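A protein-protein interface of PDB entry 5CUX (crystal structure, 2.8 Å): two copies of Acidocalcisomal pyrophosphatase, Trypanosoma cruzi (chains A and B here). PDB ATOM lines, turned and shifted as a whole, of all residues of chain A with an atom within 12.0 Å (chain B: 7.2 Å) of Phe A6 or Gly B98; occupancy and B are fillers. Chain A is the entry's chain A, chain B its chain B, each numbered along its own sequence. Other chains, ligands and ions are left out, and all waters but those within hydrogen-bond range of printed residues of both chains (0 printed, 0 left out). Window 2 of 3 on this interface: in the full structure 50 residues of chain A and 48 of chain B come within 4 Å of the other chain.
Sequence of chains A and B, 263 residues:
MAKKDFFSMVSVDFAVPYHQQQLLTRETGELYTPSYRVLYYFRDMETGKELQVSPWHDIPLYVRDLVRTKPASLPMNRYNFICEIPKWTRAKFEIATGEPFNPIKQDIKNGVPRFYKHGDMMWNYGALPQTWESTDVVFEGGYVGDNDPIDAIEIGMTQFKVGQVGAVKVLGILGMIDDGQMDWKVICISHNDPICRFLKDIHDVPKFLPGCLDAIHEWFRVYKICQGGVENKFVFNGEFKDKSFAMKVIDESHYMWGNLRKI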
ATOM      1  N   MET A   1     -16.229   8.580  39.972  1.00  0.00           N
ATOM      2  CA  MET A   1     -16.951   7.276  39.811  1.00  0.00           C
ATOM      3  C   MET A   1     -17.876   7.365  38.566  1.00  0.00           C
ATOM      4  O   MET A   1     -18.865   6.638  38.443  1.00  0.00           O
ATOM      5  CB  MET A   1     -17.725   6.915  41.127  1.00  0.00           C
ATOM      6  CG  MET A   1     -16.785   6.345  42.259  1.00  0.00           C
ATOM      7  SD  MET A   1     -17.268   6.174  44.132  1.00  0.00           S
ATOM      8  CE  MET A   1     -15.772   6.840  45.018  1.00  0.00           C
ATOM      9  N   ALA A   2     -17.525   8.242  37.623  1.00  0.00           N
ATOM     10  CA  ALA A   2     -18.318   8.424  36.396  1.00  0.00           C
ATOM     11  C   ALA A   2     -18.152   7.291  35.395  1.00  0.00           C
ATOM     12  O   ALA A   2     -17.911   7.549  34.209  1.00  0.00           O
ATOM     13  CB  ALA A   2     -17.980   9.769  35.712  1.00  0.00           C
ATOM     14  N   LYS A   3     -18.281   6.042  35.868  1.00  0.00           N
ATOM     15  CA  LYS A   3     -18.172   4.873  34.973  1.00  0.00           C
ATOM     16  C   LYS A   3     -19.297   3.820  35.014  1.00  0.00           C
ATOM     17  O   LYS A   3     -19.416   2.954  35.911  1.00  0.00           O
ATOM     18  CB  LYS A   3     -16.808   4.237  35.112  1.00  0.00           C
ATOM     19  CG  LYS A   3     -15.742   5.219  34.632  1.00  0.00           C
ATOM     20  CD  LYS A   3     -16.129   5.946  33.329  1.00  0.00           C
ATOM     21  CE  LYS A   3     -14.874   6.610  32.694  1.00  0.00           C
ATOM     22  NZ  LYS A   3     -15.010   7.491  31.480  1.00  0.00           N
ATOM     23  N   LYS A   4     -20.143   3.975  33.986  1.00  0.00           N
ATOM     24  CA  LYS A   4     -21.299   3.138  33.736  1.00  0.00           C
ATOM     25  C   LYS A   4     -21.045   2.229  32.503  1.00  0.00           C
ATOM     26  O   LYS A   4     -21.135   2.606  31.342  1.00  0.00           O
ATOM     27  CB  LYS A   4     -22.538   4.019  33.660  1.00  0.00           C
ATOM     28  CG  LYS A   4     -22.783   4.572  35.052  1.00  0.00           C
ATOM     29  CD  LYS A   4     -21.500   5.251  35.578  1.00  0.00           C
ATOM     30  CE  LYS A   4     -21.506   5.690  37.024  1.00  0.00           C
ATOM     31  NZ  LYS A   4     -22.437   6.793  37.368  1.00  0.00           N
ATOM     32  N   ASP A   5     -20.647   1.021  32.883  1.00  0.00           N
ATOM     33  CA  ASP A   5     -20.273  -0.069  32.052  1.00  0.00           C
ATOM     34  C   ASP A   5     -21.333  -1.121  32.205  1.00  0.00           C
ATOM     35  O   ASP A   5     -21.275  -1.940  33.123  1.00  0.00           O
ATOM     36  CB  ASP A   5     -18.972  -0.692  32.556  1.00  0.00           C
ATOM     37  CG  ASP A   5     -17.946   0.328  32.947  1.00  0.00           C
ATOM     38  OD1 ASP A   5     -18.259   1.177  33.787  1.00  0.00           O
ATOM     39  OD2 ASP A   5     -16.809   0.286  32.442  1.00  0.00           O
ATOM     40  N   PHE A   6     -22.305  -1.095  31.320  1.00  0.00           N
ATOM     41  CA  PHE A   6     -23.334  -2.096  31.327  1.00  0.00           C
ATOM     42  C   PHE A   6     -23.399  -2.262  29.842  1.00  0.00           C
ATOM     43  O   PHE A   6     -23.845  -1.359  29.151  1.00  0.00           O
ATOM     44  CB  PHE A   6     -24.608  -1.512  31.913  1.00  0.00           C
ATOM     45  CG  PHE A   6     -24.425  -0.983  33.312  1.00  0.00           C
ATOM     46  CD1 PHE A   6     -24.526  -1.825  34.405  1.00  0.00           C
ATOM     47  CD2 PHE A   6     -24.066   0.342  33.524  1.00  0.00           C
ATOM     48  CE1 PHE A   6     -24.265  -1.350  35.685  1.00  0.00           C
ATOM     49  CE2 PHE A   6     -23.806   0.824  34.799  1.00  0.00           C
ATOM     50  CZ  PHE A   6     -23.904  -0.023  35.877  1.00  0.00           C
ATOM     51  N   PHE A   7     -22.879  -3.384  29.347  1.00  0.00           N
ATOM     52  CA  PHE A   7     -22.843  -3.659  27.924  1.00  0.00           C
ATOM     53  C   PHE A   7     -23.664  -4.862  27.603  1.00  0.00           C
ATOM     54  O   PHE A   7     -23.301  -5.965  27.990  1.00  0.00           O
ATOM     55  CB  PHE A   7     -21.413  -3.864  27.499  1.00  0.00           C
ATOM     56  CG  PHE A   7     -20.550  -2.731  27.885  1.00  0.00           C
ATOM     57  CD1 PHE A   7     -20.701  -1.497  27.282  1.00  0.00           C
ATOM     58  CD2 PHE A   7     -19.672  -2.837  28.957  1.00  0.00           C
ATOM     59  CE1 PHE A   7     -19.996  -0.368  27.744  1.00  0.00           C
ATOM     60  CE2 PHE A   7     -18.961  -1.719  29.432  1.00  0.00           C
ATOM     61  CZ  PHE A   7     -19.128  -0.484  28.823  1.00  0.00           C
ATOM     62  N   SER A   8     -24.780  -4.642  26.898  1.00  0.00           N
ATOM     63  CA  SER A   8     -25.671  -5.721  26.511  1.00  0.00           C
ATOM     64  C   SER A   8     -25.063  -6.534  25.402  1.00  0.00           C
ATOM     65  O   SER A   8     -24.659  -5.992  24.404  1.00  0.00           O
ATOM     66  CB  SER A   8     -27.018  -5.183  26.062  1.00  0.00           C
ATOM     67  OG  SER A   8     -27.857  -6.262  25.659  1.00  0.00           O
ATOM     68  N   MET A   9     -24.998  -7.843  25.607  1.00  0.00           N
ATOM     69  CA  MET A   9     -24.431  -8.768  24.647  1.00  0.00           C
ATOM     70  C   MET A   9     -25.534  -9.483  23.886  1.00  0.00           C
ATOM     71  O   MET A   9     -25.233 -10.359  23.086  1.00  0.00           O
ATOM     72  CB  MET A   9     -23.567  -9.820  25.334  1.00  0.00           C
ATOM     73  CG  MET A   9     -22.436  -9.306  26.188  1.00  0.00           C
ATOM     74  SD  MET A   9     -21.379  -8.161  25.323  1.00  0.00           S
ATOM     75  CE  MET A   9     -21.131  -9.107  23.975  1.00  0.00           C
ATOM     76  N   VAL A  10     -26.802  -9.135  24.134  1.00  0.00           N
ATOM     77  CA  VAL A  10     -27.936  -9.749  23.413  1.00  0.00           C
ATOM     78  C   VAL A  10     -27.705  -9.639  21.903  1.00  0.00           C
ATOM     79  O   VAL A  10     -27.483  -8.538  21.383  1.00  0.00           O
ATOM     80  CB  VAL A  10     -29.247  -9.027  23.732  1.00  0.00           C
ATOM     81  CG1 VAL A  10     -30.395  -9.619  22.963  1.00  0.00           C
ATOM     82  CG2 VAL A  10     -29.493  -9.093  25.199  1.00  0.00           C
ATOM     83  N   SER A  11     -27.765 -10.761  21.205  1.00  0.00           N
ATOM     84  CA  SER A  11     -27.523 -10.758  19.778  1.00  0.00           C
ATOM     85  C   SER A  11     -28.198 -11.975  19.204  1.00  0.00           C
ATOM     86  O   SER A  11     -28.463 -12.916  19.937  1.00  0.00           O
ATOM     87  CB  SER A  11     -26.023 -10.868  19.506  1.00  0.00           C
ATOM     88  OG  SER A  11     -25.661 -12.199  19.156  1.00  0.00           O
ATOM     89  N   TRP B  56     -24.342  -3.645  16.442  1.00  0.00           N
ATOM     90  CA  TRP B  56     -22.980  -3.820  16.926  1.00  0.00           C
ATOM     91  C   TRP B  56     -22.418  -5.250  16.884  1.00  0.00           C
ATOM     92  O   TRP B  56     -21.316  -5.471  16.382  1.00  0.00           O
ATOM     93  CB  TRP B  56     -22.904  -3.275  18.342  1.00  0.00           C
ATOM     94  CG  TRP B  56     -21.626  -3.408  19.085  1.00  0.00           C
ATOM     95  CD1 TRP B  56     -20.358  -3.447  18.579  1.00  0.00           C
ATOM     96  CD2 TRP B  56     -21.491  -3.420  20.496  1.00  0.00           C
ATOM     97  NE1 TRP B  56     -19.430  -3.483  19.600  1.00  0.00           N
ATOM     98  CE2 TRP B  56     -20.106  -3.473  20.791  1.00  0.00           C
ATOM     99  CE3 TRP B  56     -22.402  -3.388  21.550  1.00  0.00           C
ATOM    100  CZ2 TRP B  56     -19.622  -3.504  22.105  1.00  0.00           C
ATOM    101  CZ3 TRP B  56     -21.914  -3.417  22.855  1.00  0.00           C
ATOM    102  CH2 TRP B  56     -20.544  -3.479  23.120  1.00  0.00           C
ATOM    103  N   ILE B  95     -25.003   4.382  19.461  1.00  0.00           N
ATOM    104  CA  ILE B  95     -25.493   3.031  19.639  1.00  0.00           C
ATOM    105  C   ILE B  95     -25.696   2.841  21.145  1.00  0.00           C
ATOM    106  O   ILE B  95     -24.834   3.167  21.916  1.00  0.00           O
ATOM    107  CB  ILE B  95     -24.482   1.979  19.113  1.00  0.00           C
ATOM    108  CG1 ILE B  95     -24.295   2.172  17.594  1.00  0.00           C
ATOM    109  CG2 ILE B  95     -24.990   0.535  19.489  1.00  0.00           C
ATOM    110  CD1 ILE B  95     -23.290   1.239  16.963  1.00  0.00           C
ATOM    111  N   ALA B  96     -26.846   2.348  21.570  1.00  0.00           N
ATOM    112  CA  ALA B  96     -27.074   2.108  23.005  1.00  0.00           C
ATOM    113  C   ALA B  96     -26.399   0.772  23.384  1.00  0.00           C
ATOM    114  O   ALA B  96     -27.032  -0.303  23.312  1.00  0.00           O
ATOM    115  CB  ALA B  96     -28.580   2.042  23.297  1.00  0.00           C
ATOM    116  N   THR B  97     -25.110   0.824  23.739  1.00  0.00           N
ATOM    117  CA  THR B  97     -24.381  -0.385  24.092  1.00  0.00           C
ATOM    118  C   THR B  97     -24.995  -1.045  25.342  1.00  0.00           C
ATOM    119  O   THR B  97     -24.701  -2.200  25.637  1.00  0.00           O
ATOM    120  CB  THR B  97     -22.910  -0.081  24.325  1.00  0.00           C
ATOM    121  OG1 THR B  97     -22.767   0.927  25.316  1.00  0.00           O
ATOM    122  CG2 THR B  97     -22.276   0.438  23.086  1.00  0.00           C
ATOM    123  N   GLY B  98     -25.879  -0.320  26.046  1.00  0.00           N
ATOM    124  CA  GLY B  98     -26.522  -0.841  27.234  1.00  0.00           C
ATOM    125  C   GLY B  98     -27.873  -1.506  27.027  1.00  0.00           C
ATOM    126  O   GLY B  98     -28.261  -2.400  27.794  1.00  0.00           O
ATOM    127  N   GLU B  99     -28.608  -1.087  26.004  1.00  0.00           N
ATOM    128  CA  GLU B  99     -29.920  -1.653  25.715  1.00  0.00           C
ATOM    129  C   GLU B  99     -29.828  -2.923  24.874  1.00  0.00           C
ATOM    130  O   GLU B  99     -28.939  -3.060  24.044  1.00  0.00           O
ATOM    131  CB  GLU B  99     -30.758  -0.622  24.982  1.00  0.00           C
ATOM    132  CG  GLU B  99     -30.875   0.633  25.755  1.00  0.00           C
ATOM    133  CD  GLU B  99     -31.662   1.698  25.042  1.00  0.00           C
ATOM    134  OE1 GLU B  99     -32.359   1.376  24.049  1.00  0.00           O
ATOM    135  OE2 GLU B  99     -31.574   2.862  25.505  1.00  0.00           O
ATOM    136  N   PRO B 100     -30.765  -3.860  25.069  1.00  0.00           N
ATOM    137  CA  PRO B 100     -30.825  -5.139  24.348  1.00  0.00           C
ATOM    138  C   PRO B 100     -30.893  -4.905  22.868  1.00  0.00           C
ATOM    139  O   PRO B 100     -31.705  -4.118  22.438  1.00  0.00           O
ATOM    140  CB  PRO B 100     -32.116  -5.766  24.851  1.00  0.00           C
ATOM    141  CG  PRO B 100     -32.287  -5.180  26.187  1.00  0.00           C
ATOM    142  CD  PRO B 100     -31.888  -3.738  26.007  1.00  0.00           C
ATOM    143  N   PHE B 101     -30.067  -5.584  22.082  1.00  0.00           N
ATOM    144  CA  PHE B 101     -30.079  -5.388  20.621  1.00  0.00           C
ATOM    145  C   PHE B 101     -29.547  -4.019  20.173  1.00  0.00           C
ATOM    146  O   PHE B 101     -29.858  -3.539  19.091  1.00  0.00           O
ATOM    147  CB  PHE B 101     -31.481  -5.598  20.057  1.00  0.00           C
ATOM    148  CG  PHE B 101     -31.935  -7.022  20.092  1.00  0.00           C
ATOM    149  CD1 PHE B 101     -31.192  -8.011  19.456  1.00  0.00           C
ATOM    150  CD2 PHE B 101     -33.103  -7.383  20.767  1.00  0.00           C
ATOM    151  CE1 PHE B 101     -31.597  -9.338  19.488  1.00  0.00           C
ATOM    152  CE2 PHE B 101     -33.520  -8.713  20.802  1.00  0.00           C
ATOM    153  CZ  PHE B 101     -32.758  -9.689  20.159  1.00  0.00           C
ATOM    154  N   ASN B 102     -28.767  -3.394  21.037  1.00  0.00           N
ATOM    155  CA  ASN B 102     -28.106  -2.133  20.778  1.00  0.00           C
ATOM    156  C   ASN B 102     -28.639  -1.206  19.669  1.00  0.00           C
ATOM    157  O   ASN B 102     -27.925  -0.899  18.714  1.00  0.00           O
ATOM    158  CB  ASN B 102     -26.637  -2.482  20.545  1.00  0.00           C
ATOM    159  CG  ASN B 102     -26.121  -3.461  21.593  1.00  0.00           C
ATOM    160  OD1 ASN B 102     -26.015  -4.671  21.368  1.00  0.00           O
ATOM    161  ND2 ASN B 102     -25.845  -2.929  22.784  1.00  0.00           N
ATOM    162  N   PRO B 103     -29.886  -0.714  19.800  1.00  0.00           N
ATOM    163  CA  PRO B 103     -30.488   0.178  18.808  1.00  0.00           C
ATOM    164  C   PRO B 103     -29.859   1.543  18.908  1.00  0.00           C
ATOM    165  O   PRO B 103     -29.130   1.824  19.850  1.00  0.00           O
ATOM    166  CB  PRO B 103     -31.932   0.220  19.237  1.00  0.00           C
ATOM    167  CG  PRO B 103     -31.773   0.243  20.680  1.00  0.00           C
ATOM    168  CD  PRO B 103     -30.797  -0.868  20.939  1.00  0.00           C
ATOM    169  N   LYS B 105     -29.953   5.408  19.670  1.00  0.00           N
ATOM    170  CA  LYS B 105     -30.756   6.334  20.436  1.00  0.00           C
ATOM    171  C   LYS B 105     -30.042   7.671  20.472  1.00  0.00           C
ATOM    172  O   LYS B 105     -28.860   7.739  20.181  1.00  0.00           O
ATOM    173  CB  LYS B 105     -30.973   5.809  21.857  1.00  0.00           C
ATOM    174  CG  LYS B 105     -29.836   6.038  22.886  1.00  0.00           C
ATOM    175  CD  LYS B 105     -30.175   5.190  24.109  1.00  0.00           C
ATOM    176  CE  LYS B 105     -29.095   5.151  25.195  1.00  0.00           C
ATOM    177  NZ  LYS B 105     -28.669   6.538  25.582  1.00  0.00           N
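The backbone carbonyl oxygen (O) of Thr B97 sits at hydrogen-bond distance from the backbone NH (N) of Ser A8 (2.7 Å).
Of the 11 printed residues of chain A, 4 touch a printed residue of chain B.
Of the 11 printed residues of chain B, 6 touch a printed residue of chain A.
Among the printed residues, 9 pairs touch across the chains.
Among the printed residues, no Asp or Glu carboxylate lies within 4 Å of a Lys or Arg side-chain nitrogen of the other chain.
No position is printed for both chains.
OG of Ser A8 sits close to N of Val A10, at 3.4 Å.
The backbone carbonyl oxygen (O) of Ala B96 is in hydrogen-bond range of the side-chain amide nitrogen (ND2) of Asn B102 (2.9 Å).
The backbone carbonyl oxygen (O) of Thr B97 sits at hydrogen-bond distance from the side-chain amide nitrogen (ND2) of Asn B102 (3.2 Å).
The side-chain amide nitrogen of Asn B102 lies within hydrogen-bond range of the backbone carbonyl oxygen of Glu B99 (3.3 Å).
Of chain B, only Thr B97 (3.7 Å) and Gly B98 (3.3 Å) come within 4 Å of Phe A6.
Of the printed residues of chain A, Gly B98 touches Phe A6 (3.3 Å) and Ser A8 (3.5 Å).
No residue of chain A comes within 4 Å of Ala B96.
Thr B97 touches just these residues of chain A: Phe A6, Phe A7 and Ser A8.
Of chain A, only Ser A8 comes within 4 Å of Pro B100.
Of chain A, only Ser A8 comes within 4 Å of Asn B102.
Of the printed residues of chain B, Ser A8 touches Thr B97 (2.7 Å), Gly B98 (3.5 Å), Glu B99 (3.5 Å), Pro B100 (3.4 Å) and Asn B102 (3.6 Å).
Of the printed residues of chain B, Val A10 touches Phe B101.
Of the printed residues of chain A, Phe B101 touches Val A10.
Trp B56 touches none of the printed residues of chain A.
Ile B95 touches none of the printed residues of chain A.
The nearest residue of chain B that does not touch Phe A6 is Glu B99 (5.7 Å).
O of Thr B97 touches O of Phe A6, 3.7 Å away.
CA of Gly B98 touches O of Phe A6 (3.3 Å).
Phe A7 touches Thr B97.
O of Gly B98 touches CB of Ser A8, 3.5 Å away.
O of Glu B99 touches CB of Ser A8 (3.5 Å).
Ser A8 touches Pro B100.
Ser A8 touches Asn B102 (O to OD1, 3.6 Å).
Val A10 touches Phe B101 (CG1 to CZ, 3.7 Å).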
